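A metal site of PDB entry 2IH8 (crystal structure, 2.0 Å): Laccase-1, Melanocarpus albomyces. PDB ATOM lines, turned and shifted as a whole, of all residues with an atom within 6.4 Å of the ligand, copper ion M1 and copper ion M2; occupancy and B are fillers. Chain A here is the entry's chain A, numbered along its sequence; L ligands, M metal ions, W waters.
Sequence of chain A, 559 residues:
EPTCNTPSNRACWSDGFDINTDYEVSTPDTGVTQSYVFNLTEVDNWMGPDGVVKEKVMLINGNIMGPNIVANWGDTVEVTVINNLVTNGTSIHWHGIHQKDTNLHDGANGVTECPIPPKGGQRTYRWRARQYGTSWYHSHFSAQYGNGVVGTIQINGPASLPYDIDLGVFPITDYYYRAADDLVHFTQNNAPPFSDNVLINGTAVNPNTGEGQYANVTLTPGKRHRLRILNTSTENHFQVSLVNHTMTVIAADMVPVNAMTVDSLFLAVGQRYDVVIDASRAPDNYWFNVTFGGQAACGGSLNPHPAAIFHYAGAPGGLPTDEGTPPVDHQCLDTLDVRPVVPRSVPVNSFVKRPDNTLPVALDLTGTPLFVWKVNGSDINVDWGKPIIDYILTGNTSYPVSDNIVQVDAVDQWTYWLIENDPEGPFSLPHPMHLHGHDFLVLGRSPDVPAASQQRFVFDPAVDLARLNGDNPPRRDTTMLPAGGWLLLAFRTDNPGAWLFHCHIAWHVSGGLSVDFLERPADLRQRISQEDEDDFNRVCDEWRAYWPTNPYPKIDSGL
A ring nitrogen (NE2) of His 93 lies close to an oxygen (O2) of the ligand, at 3.3 Å.
An oxygen (O2) of the ligand sits close to a ring nitrogen (NE2) of His 434 (3.3 Å).
Hydrophobic or aromatic side chains that line the ligand: His 93, His 95, His 138, His 140, His 434, His 502 and His 504.
Merely in contact with copper ion M1: Trp 136.
Along chain A the residues within 4 Å of copper ion M1 span positions 95 to 504.
The nearest printed residue that does not touch copper ion M1 is His 93 (4.02 Å).
His 93 touches copper ion M2 (CD2 to CU, 3.96 Å).
His 434 touches copper ion M2.
Five residues have an atom within 4 Å of copper ion M2: His 93, His 140, His 434, His 436 and His 502.
The nearest printed residue that does not touch copper ion M2 is Leu 500 (4.5 Å).
Copper ion M2 is bound by a ring nitrogen (NE2) of His 502 (1.9 Å).
NE2 of His 436 is bound to copper ion M2 (1.9 Å).
A ring nitrogen (NE2) of His 140 is bound to copper ion M2 (2.0 Å).
Copper ion M2 is bound by an oxygen (O1) of the ligand, at 2.2 Å.
The backbone NH (N) of His 434 sits at hydrogen-bond distance from the backbone carbonyl oxygen (O) of His 502, at 2.7 Å.
N of His 436 is in hydrogen-bond range of O of Leu 500 (2.9 Å).
ND1 of His 436 sits at hydrogen-bond distance from OD2 of Asp 106 (2.7 Å).
N of His 95 sits at hydrogen-bond distance from O of Trp 136 (2.9 Å).
A ring nitrogen (NE2) of His 95 lies within hydrogen-bond range of the backbone carbonyl oxygen of Gly 270, at 3.4 Å.
A ring nitrogen (ND1) of His 140 is in hydrogen-bond range of the chain-end carboxylate (OXT) of Leu 559, at 2.9 Å.
A ring nitrogen (ND1) of His 504 sits at hydrogen-bond distance from the side-chain hydroxyl of Tyr 145, at 3.1 Å.
A ring nitrogen (ND1) of His 93 is in hydrogen-bond range of the backbone carbonyl oxygen (O) of Asp 106 (2.7 Å).
Copper ion M1 is bound by a ring nitrogen (ND1) of His 95 (1.9 Å).
NE2 of His 138 is bound to copper ion M1 (2.0 Å).
Copper ion M1 is bound by a ring nitrogen (NE2) of His 504, 2.0 Å away.
O2 of the ligand binds copper ion M1, at 2.3 Å.
Copper ion M1 has four donor atoms within binding distance.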
ATOM      1  N   HIS A  93     -23.149   3.455 -30.317  1.00  0.00           N
ATOM      2  CA  HIS A  93     -22.954   4.396 -29.227  1.00  0.00           C
ATOM      3  C   HIS A  93     -23.416   5.769 -29.670  1.00  0.00           C
ATOM      4  O   HIS A  93     -23.121   6.202 -30.770  1.00  0.00           O
ATOM      5  CB  HIS A  93     -21.476   4.422 -28.787  1.00  0.00           C
ATOM      6  CG  HIS A  93     -21.161   5.507 -27.799  1.00  0.00           C
ATOM      7  ND1 HIS A  93     -21.869   5.680 -26.634  1.00  0.00           N
ATOM      8  CD2 HIS A  93     -20.239   6.491 -27.829  1.00  0.00           C
ATOM      9  CE1 HIS A  93     -21.406   6.751 -25.992  1.00  0.00           C
ATOM     10  NE2 HIS A  93     -20.410   7.254 -26.702  1.00  0.00           N
ATOM     11  N   HIS A  95     -22.707   9.142 -29.051  1.00  0.00           N
ATOM     12  CA  HIS A  95     -21.669  10.058 -28.592  1.00  0.00           C
ATOM     13  C   HIS A  95     -22.230  11.456 -28.278  1.00  0.00           C
ATOM     14  O   HIS A  95     -22.694  12.156 -29.173  1.00  0.00           O
ATOM     15  CB  HIS A  95     -20.571  10.116 -29.664  1.00  0.00           C
ATOM     16  CG  HIS A  95     -19.327  10.854 -29.253  1.00  0.00           C
ATOM     17  ND1 HIS A  95     -18.068  10.322 -29.415  1.00  0.00           N
ATOM     18  CD2 HIS A  95     -19.146  12.108 -28.775  1.00  0.00           C
ATOM     19  CE1 HIS A  95     -17.173  11.215 -29.052  1.00  0.00           C
ATOM     20  NE2 HIS A  95     -17.799  12.309 -28.660  1.00  0.00           N
ATOM     21  N   GLY A  96     -22.058  11.867 -27.031  1.00  0.00           N
ATOM     22  CA  GLY A  96     -22.524  13.164 -26.584  1.00  0.00           C
ATOM     23  C   GLY A  96     -23.833  13.087 -25.831  1.00  0.00           C
ATOM     24  O   GLY A  96     -24.207  14.021 -25.128  1.00  0.00           O
ATOM     25  N   ASP A 106     -26.277   2.882 -23.820  1.00  0.00           N
ATOM     26  CA  ASP A 106     -25.055   3.592 -24.219  1.00  0.00           C
ATOM     27  C   ASP A 106     -24.366   3.029 -25.467  1.00  0.00           C
ATOM     28  O   ASP A 106     -23.681   3.761 -26.171  1.00  0.00           O
ATOM     29  CB  ASP A 106     -24.083   3.655 -23.043  1.00  0.00           C
ATOM     30  CG  ASP A 106     -22.957   4.656 -23.261  1.00  0.00           C
ATOM     31  OD1 ASP A 106     -23.243   5.826 -23.587  1.00  0.00           O
ATOM     32  OD2 ASP A 106     -21.778   4.253 -23.113  1.00  0.00           O
ATOM     33  N   ALA A 108     -22.033   0.606 -25.563  1.00  0.00           N
ATOM     34  CA  ALA A 108     -20.638   0.254 -25.305  1.00  0.00           C
ATOM     35  C   ALA A 108     -20.569  -1.246 -25.064  1.00  0.00           C
ATOM     36  O   ALA A 108     -20.825  -1.723 -23.958  1.00  0.00           O
ATOM     37  CB  ALA A 108     -20.130   1.024 -24.089  1.00  0.00           C
ATOM     38  N   TRP A 136     -23.164  12.798 -32.492  1.00  0.00           N
ATOM     39  CA  TRP A 136     -23.039  11.771 -33.498  1.00  0.00           C
ATOM     40  C   TRP A 136     -23.127  10.398 -32.892  1.00  0.00           C
ATOM     41  O   TRP A 136     -23.177  10.255 -31.666  1.00  0.00           O
ATOM     42  CB  TRP A 136     -21.740  11.941 -34.315  1.00  0.00           C
ATOM     43  CG  TRP A 136     -20.430  11.778 -33.570  1.00  0.00           C
ATOM     44  CD1 TRP A 136     -20.002  12.511 -32.491  1.00  0.00           C
ATOM     45  CD2 TRP A 136     -19.361  10.898 -33.907  1.00  0.00           C
ATOM     46  NE1 TRP A 136     -18.715  12.138 -32.149  1.00  0.00           N
ATOM     47  CE2 TRP A 136     -18.296  11.146 -33.006  1.00  0.00           C
ATOM     48  CE3 TRP A 136     -19.195   9.913 -34.900  1.00  0.00           C
ATOM     49  CZ2 TRP A 136     -17.071  10.458 -33.066  1.00  0.00           C
ATOM     50  CZ3 TRP A 136     -17.951   9.214 -34.970  1.00  0.00           C
ATOM     51  CH2 TRP A 136     -16.906   9.501 -34.052  1.00  0.00           C
ATOM     52  N   HIS A 138     -21.918   6.101 -33.531  1.00  0.00           N
ATOM     53  CA  HIS A 138     -20.969   5.205 -34.164  1.00  0.00           C
ATOM     54  C   HIS A 138     -20.907   3.863 -33.469  1.00  0.00           C
ATOM     55  O   HIS A 138     -21.308   3.735 -32.313  1.00  0.00           O
ATOM     56  CB  HIS A 138     -19.561   5.852 -34.187  1.00  0.00           C
ATOM     57  CG  HIS A 138     -18.981   6.136 -32.827  1.00  0.00           C
ATOM     58  ND1 HIS A 138     -18.340   5.175 -32.079  1.00  0.00           N
ATOM     59  CD2 HIS A 138     -18.912   7.279 -32.102  1.00  0.00           C
ATOM     60  CE1 HIS A 138     -17.896   5.713 -30.958  1.00  0.00           C
ATOM     61  NE2 HIS A 138     -18.220   6.993 -30.949  1.00  0.00           N
ATOM     62  N   SER A 139     -20.366   2.875 -34.166  1.00  0.00           N
ATOM     63  CA  SER A 139     -20.197   1.543 -33.597  1.00  0.00           C
ATOM     64  C   SER A 139     -19.055   1.615 -32.584  1.00  0.00           C
ATOM     65  O   SER A 139     -18.139   2.428 -32.736  1.00  0.00           O
ATOM     66  CB  SER A 139     -19.843   0.531 -34.676  1.00  0.00           C
ATOM     67  OG  SER A 139     -19.554  -0.739 -34.101  1.00  0.00           O
ATOM     68  N   HIS A 140     -19.171   0.799 -31.533  1.00  0.00           N
ATOM     69  CA  HIS A 140     -18.117   0.714 -30.525  1.00  0.00           C
ATOM     70  C   HIS A 140     -17.520  -0.697 -30.554  1.00  0.00           C
ATOM     71  O   HIS A 140     -16.791  -1.098 -29.638  1.00  0.00           O
ATOM     72  CB  HIS A 140     -18.644   1.081 -29.138  1.00  0.00           C
ATOM     73  CG  HIS A 140     -17.790   2.085 -28.416  1.00  0.00           C
ATOM     74  ND1 HIS A 140     -16.425   1.942 -28.276  1.00  0.00           N
ATOM     75  CD2 HIS A 140     -18.097   3.256 -27.810  1.00  0.00           C
ATOM     76  CE1 HIS A 140     -15.934   2.976 -27.631  1.00  0.00           C
ATOM     77  NE2 HIS A 140     -16.934   3.796 -27.333  1.00  0.00           N
ATOM     78  N   TYR A 145     -16.503   1.422 -36.790  1.00  0.00           N
ATOM     79  CA  TYR A 145     -17.025   2.681 -37.305  1.00  0.00           C
ATOM     80  C   TYR A 145     -16.167   3.260 -38.433  1.00  0.00           C
ATOM     81  O   TYR A 145     -16.638   4.047 -39.247  1.00  0.00           O
ATOM     82  CB  TYR A 145     -17.333   3.683 -36.183  1.00  0.00           C
ATOM     83  CG  TYR A 145     -16.224   4.592 -35.664  1.00  0.00           C
ATOM     84  CD1 TYR A 145     -15.948   5.832 -36.293  1.00  0.00           C
ATOM     85  CD2 TYR A 145     -15.538   4.293 -34.467  1.00  0.00           C
ATOM     86  CE1 TYR A 145     -15.022   6.763 -35.746  1.00  0.00           C
ATOM     87  CE2 TYR A 145     -14.608   5.221 -33.906  1.00  0.00           C
ATOM     88  CZ  TYR A 145     -14.356   6.443 -34.555  1.00  0.00           C
ATOM     89  OH  TYR A 145     -13.467   7.350 -34.032  1.00  0.00           O
ATOM     90  N   GLY A 270     -14.056  13.303 -32.592  1.00  0.00           N
ATOM     91  CA  GLY A 270     -15.261  13.254 -31.797  1.00  0.00           C
ATOM     92  C   GLY A 270     -15.831  14.605 -31.393  1.00  0.00           C
ATOM     93  O   GLY A 270     -16.948  14.671 -30.890  1.00  0.00           O
ATOM     94  N   HIS A 434     -12.221  11.289 -24.380  1.00  0.00           N
ATOM     95  CA  HIS A 434     -13.673  11.349 -24.389  1.00  0.00           C
ATOM     96  C   HIS A 434     -14.288  10.591 -23.222  1.00  0.00           C
ATOM     97  O   HIS A 434     -13.851   9.491 -22.890  1.00  0.00           O
ATOM     98  CB  HIS A 434     -14.194  10.798 -25.733  1.00  0.00           C
ATOM     99  CG  HIS A 434     -15.669  10.609 -25.779  1.00  0.00           C
ATOM    100  ND1 HIS A 434     -16.566  11.635 -25.545  1.00  0.00           N
ATOM    101  CD2 HIS A 434     -16.422   9.496 -25.972  1.00  0.00           C
ATOM    102  CE1 HIS A 434     -17.793  11.159 -25.582  1.00  0.00           C
ATOM    103  NE2 HIS A 434     -17.734   9.867 -25.844  1.00  0.00           N
ATOM    104  N   HIS A 436     -17.945   9.024 -21.593  1.00  0.00           N
ATOM    105  CA  HIS A 436     -19.313   8.599 -21.831  1.00  0.00           C
ATOM    106  C   HIS A 436     -20.173   9.033 -20.644  1.00  0.00           C
ATOM    107  O   HIS A 436     -19.676   9.158 -19.515  1.00  0.00           O
ATOM    108  CB  HIS A 436     -19.406   7.058 -21.931  1.00  0.00           C
ATOM    109  CG  HIS A 436     -18.855   6.472 -23.193  1.00  0.00           C
ATOM    110  ND1 HIS A 436     -19.360   5.304 -23.731  1.00  0.00           N
ATOM    111  CD2 HIS A 436     -17.817   6.833 -23.994  1.00  0.00           C
ATOM    112  CE1 HIS A 436     -18.655   4.971 -24.800  1.00  0.00           C
ATOM    113  NE2 HIS A 436     -17.716   5.894 -24.975  1.00  0.00           N
ATOM    114  N   LEU A 500     -17.276   4.531 -20.076  1.00  0.00           N
ATOM    115  CA  LEU A 500     -15.952   4.534 -20.669  1.00  0.00           C
ATOM    116  C   LEU A 500     -15.367   5.931 -20.774  1.00  0.00           C
ATOM    117  O   LEU A 500     -16.085   6.912 -21.006  1.00  0.00           O
ATOM    118  CB  LEU A 500     -15.976   3.922 -22.067  1.00  0.00           C
ATOM    119  CG  LEU A 500     -16.209   2.420 -22.194  1.00  0.00           C
ATOM    120  CD1 LEU A 500     -16.281   2.078 -23.673  1.00  0.00           C
ATOM    121  CD2 LEU A 500     -15.104   1.641 -21.507  1.00  0.00           C
ATOM    122  N   HIS A 502     -12.102   7.204 -22.635  1.00  0.00           N
ATOM    123  CA  HIS A 502     -11.078   6.769 -23.562  1.00  0.00           C
ATOM    124  C   HIS A 502     -10.591   7.777 -24.563  1.00  0.00           C
ATOM    125  O   HIS A 502     -11.230   8.803 -24.794  1.00  0.00           O
ATOM    126  CB  HIS A 502     -11.580   5.540 -24.326  1.00  0.00           C
ATOM    127  CG  HIS A 502     -12.802   5.784 -25.164  1.00  0.00           C
ATOM    128  ND1 HIS A 502     -12.730   6.057 -26.509  1.00  0.00           N
ATOM    129  CD2 HIS A 502     -14.126   5.757 -24.855  1.00  0.00           C
ATOM    130  CE1 HIS A 502     -13.958   6.180 -27.001  1.00  0.00           C
ATOM    131  NE2 HIS A 502     -14.816   6.003 -26.019  1.00  0.00           N
ATOM    132  N   HIS A 504     -10.254   8.845 -28.241  1.00  0.00           N
ATOM    133  CA  HIS A 504     -11.115   8.562 -29.383  1.00  0.00           C
ATOM    134  C   HIS A 504     -10.396   8.174 -30.671  1.00  0.00           C
ATOM    135  O   HIS A 504     -11.047   7.933 -31.695  1.00  0.00           O
ATOM    136  CB  HIS A 504     -12.122   9.671 -29.613  1.00  0.00           C
ATOM    137  CG  HIS A 504     -13.475   9.167 -30.008  1.00  0.00           C
ATOM    138  ND1 HIS A 504     -13.718   8.567 -31.221  1.00  0.00           N
ATOM    139  CD2 HIS A 504     -14.645   9.146 -29.333  1.00  0.00           C
ATOM    140  CE1 HIS A 504     -14.985   8.198 -31.278  1.00  0.00           C
ATOM    141  NE2 HIS A 504     -15.576   8.540 -30.146  1.00  0.00           N
ATOM    142  N   VAL A 509      -7.698   3.267 -28.673  1.00  0.00           N
ATOM    143  CA  VAL A 509      -8.704   2.605 -27.818  1.00  0.00           C
ATOM    144  C   VAL A 509      -8.713   1.100 -28.114  1.00  0.00           C
ATOM    145  O   VAL A 509      -8.916   0.286 -27.210  1.00  0.00           O
ATOM    146  CB  VAL A 509     -10.135   3.266 -27.895  1.00  0.00           C
ATOM    147  CG1 VAL A 509     -10.763   3.142 -29.281  1.00  0.00           C
ATOM    148  CG2 VAL A 509     -11.039   2.684 -26.815  1.00  0.00           C
ATOM    149  N   LEU A 559     -13.098  -2.347 -28.042  1.00  0.00           N
ATOM    150  CA  LEU A 559     -13.708  -1.018 -27.985  1.00  0.00           C
ATOM    151  C   LEU A 559     -13.202  -0.084 -29.090  1.00  0.00           C
ATOM    152  O   LEU A 559     -12.139  -0.390 -29.663  1.00  0.00           O
ATOM    153  CB  LEU A 559     -13.454  -0.381 -26.619  1.00  0.00           C
ATOM    154  CG  LEU A 559     -13.985  -1.106 -25.372  1.00  0.00           C
ATOM    155  CD1 LEU A 559     -13.435  -0.451 -24.133  1.00  0.00           C
ATOM    156  CD2 LEU A 559     -15.511  -1.146 -25.352  1.00  0.00           C
ATOM    157  OXT LEU A 559     -13.884   0.932 -29.363  1.00  0.00           O
HETATM  158  O1  LIG L   1     -16.566   6.560 -28.528  1.00  0.00           O
HETATM  159  O2  LIG L   1     -17.348   7.399 -27.959  1.00  0.00           O
HETATM  160 CU    CU M   1     -17.526   8.538 -29.980  1.00  0.00          CU
HETATM  161 CU    CU M   2     -16.622   5.551 -26.532  1.00  0.00          CU
HETATM  162 CU    CU M   3     -19.085   8.556 -26.350  1.00  0.00          CU
HETATM  163  O   HOH W   1     -14.567   4.973 -30.142  1.00  0.00           O
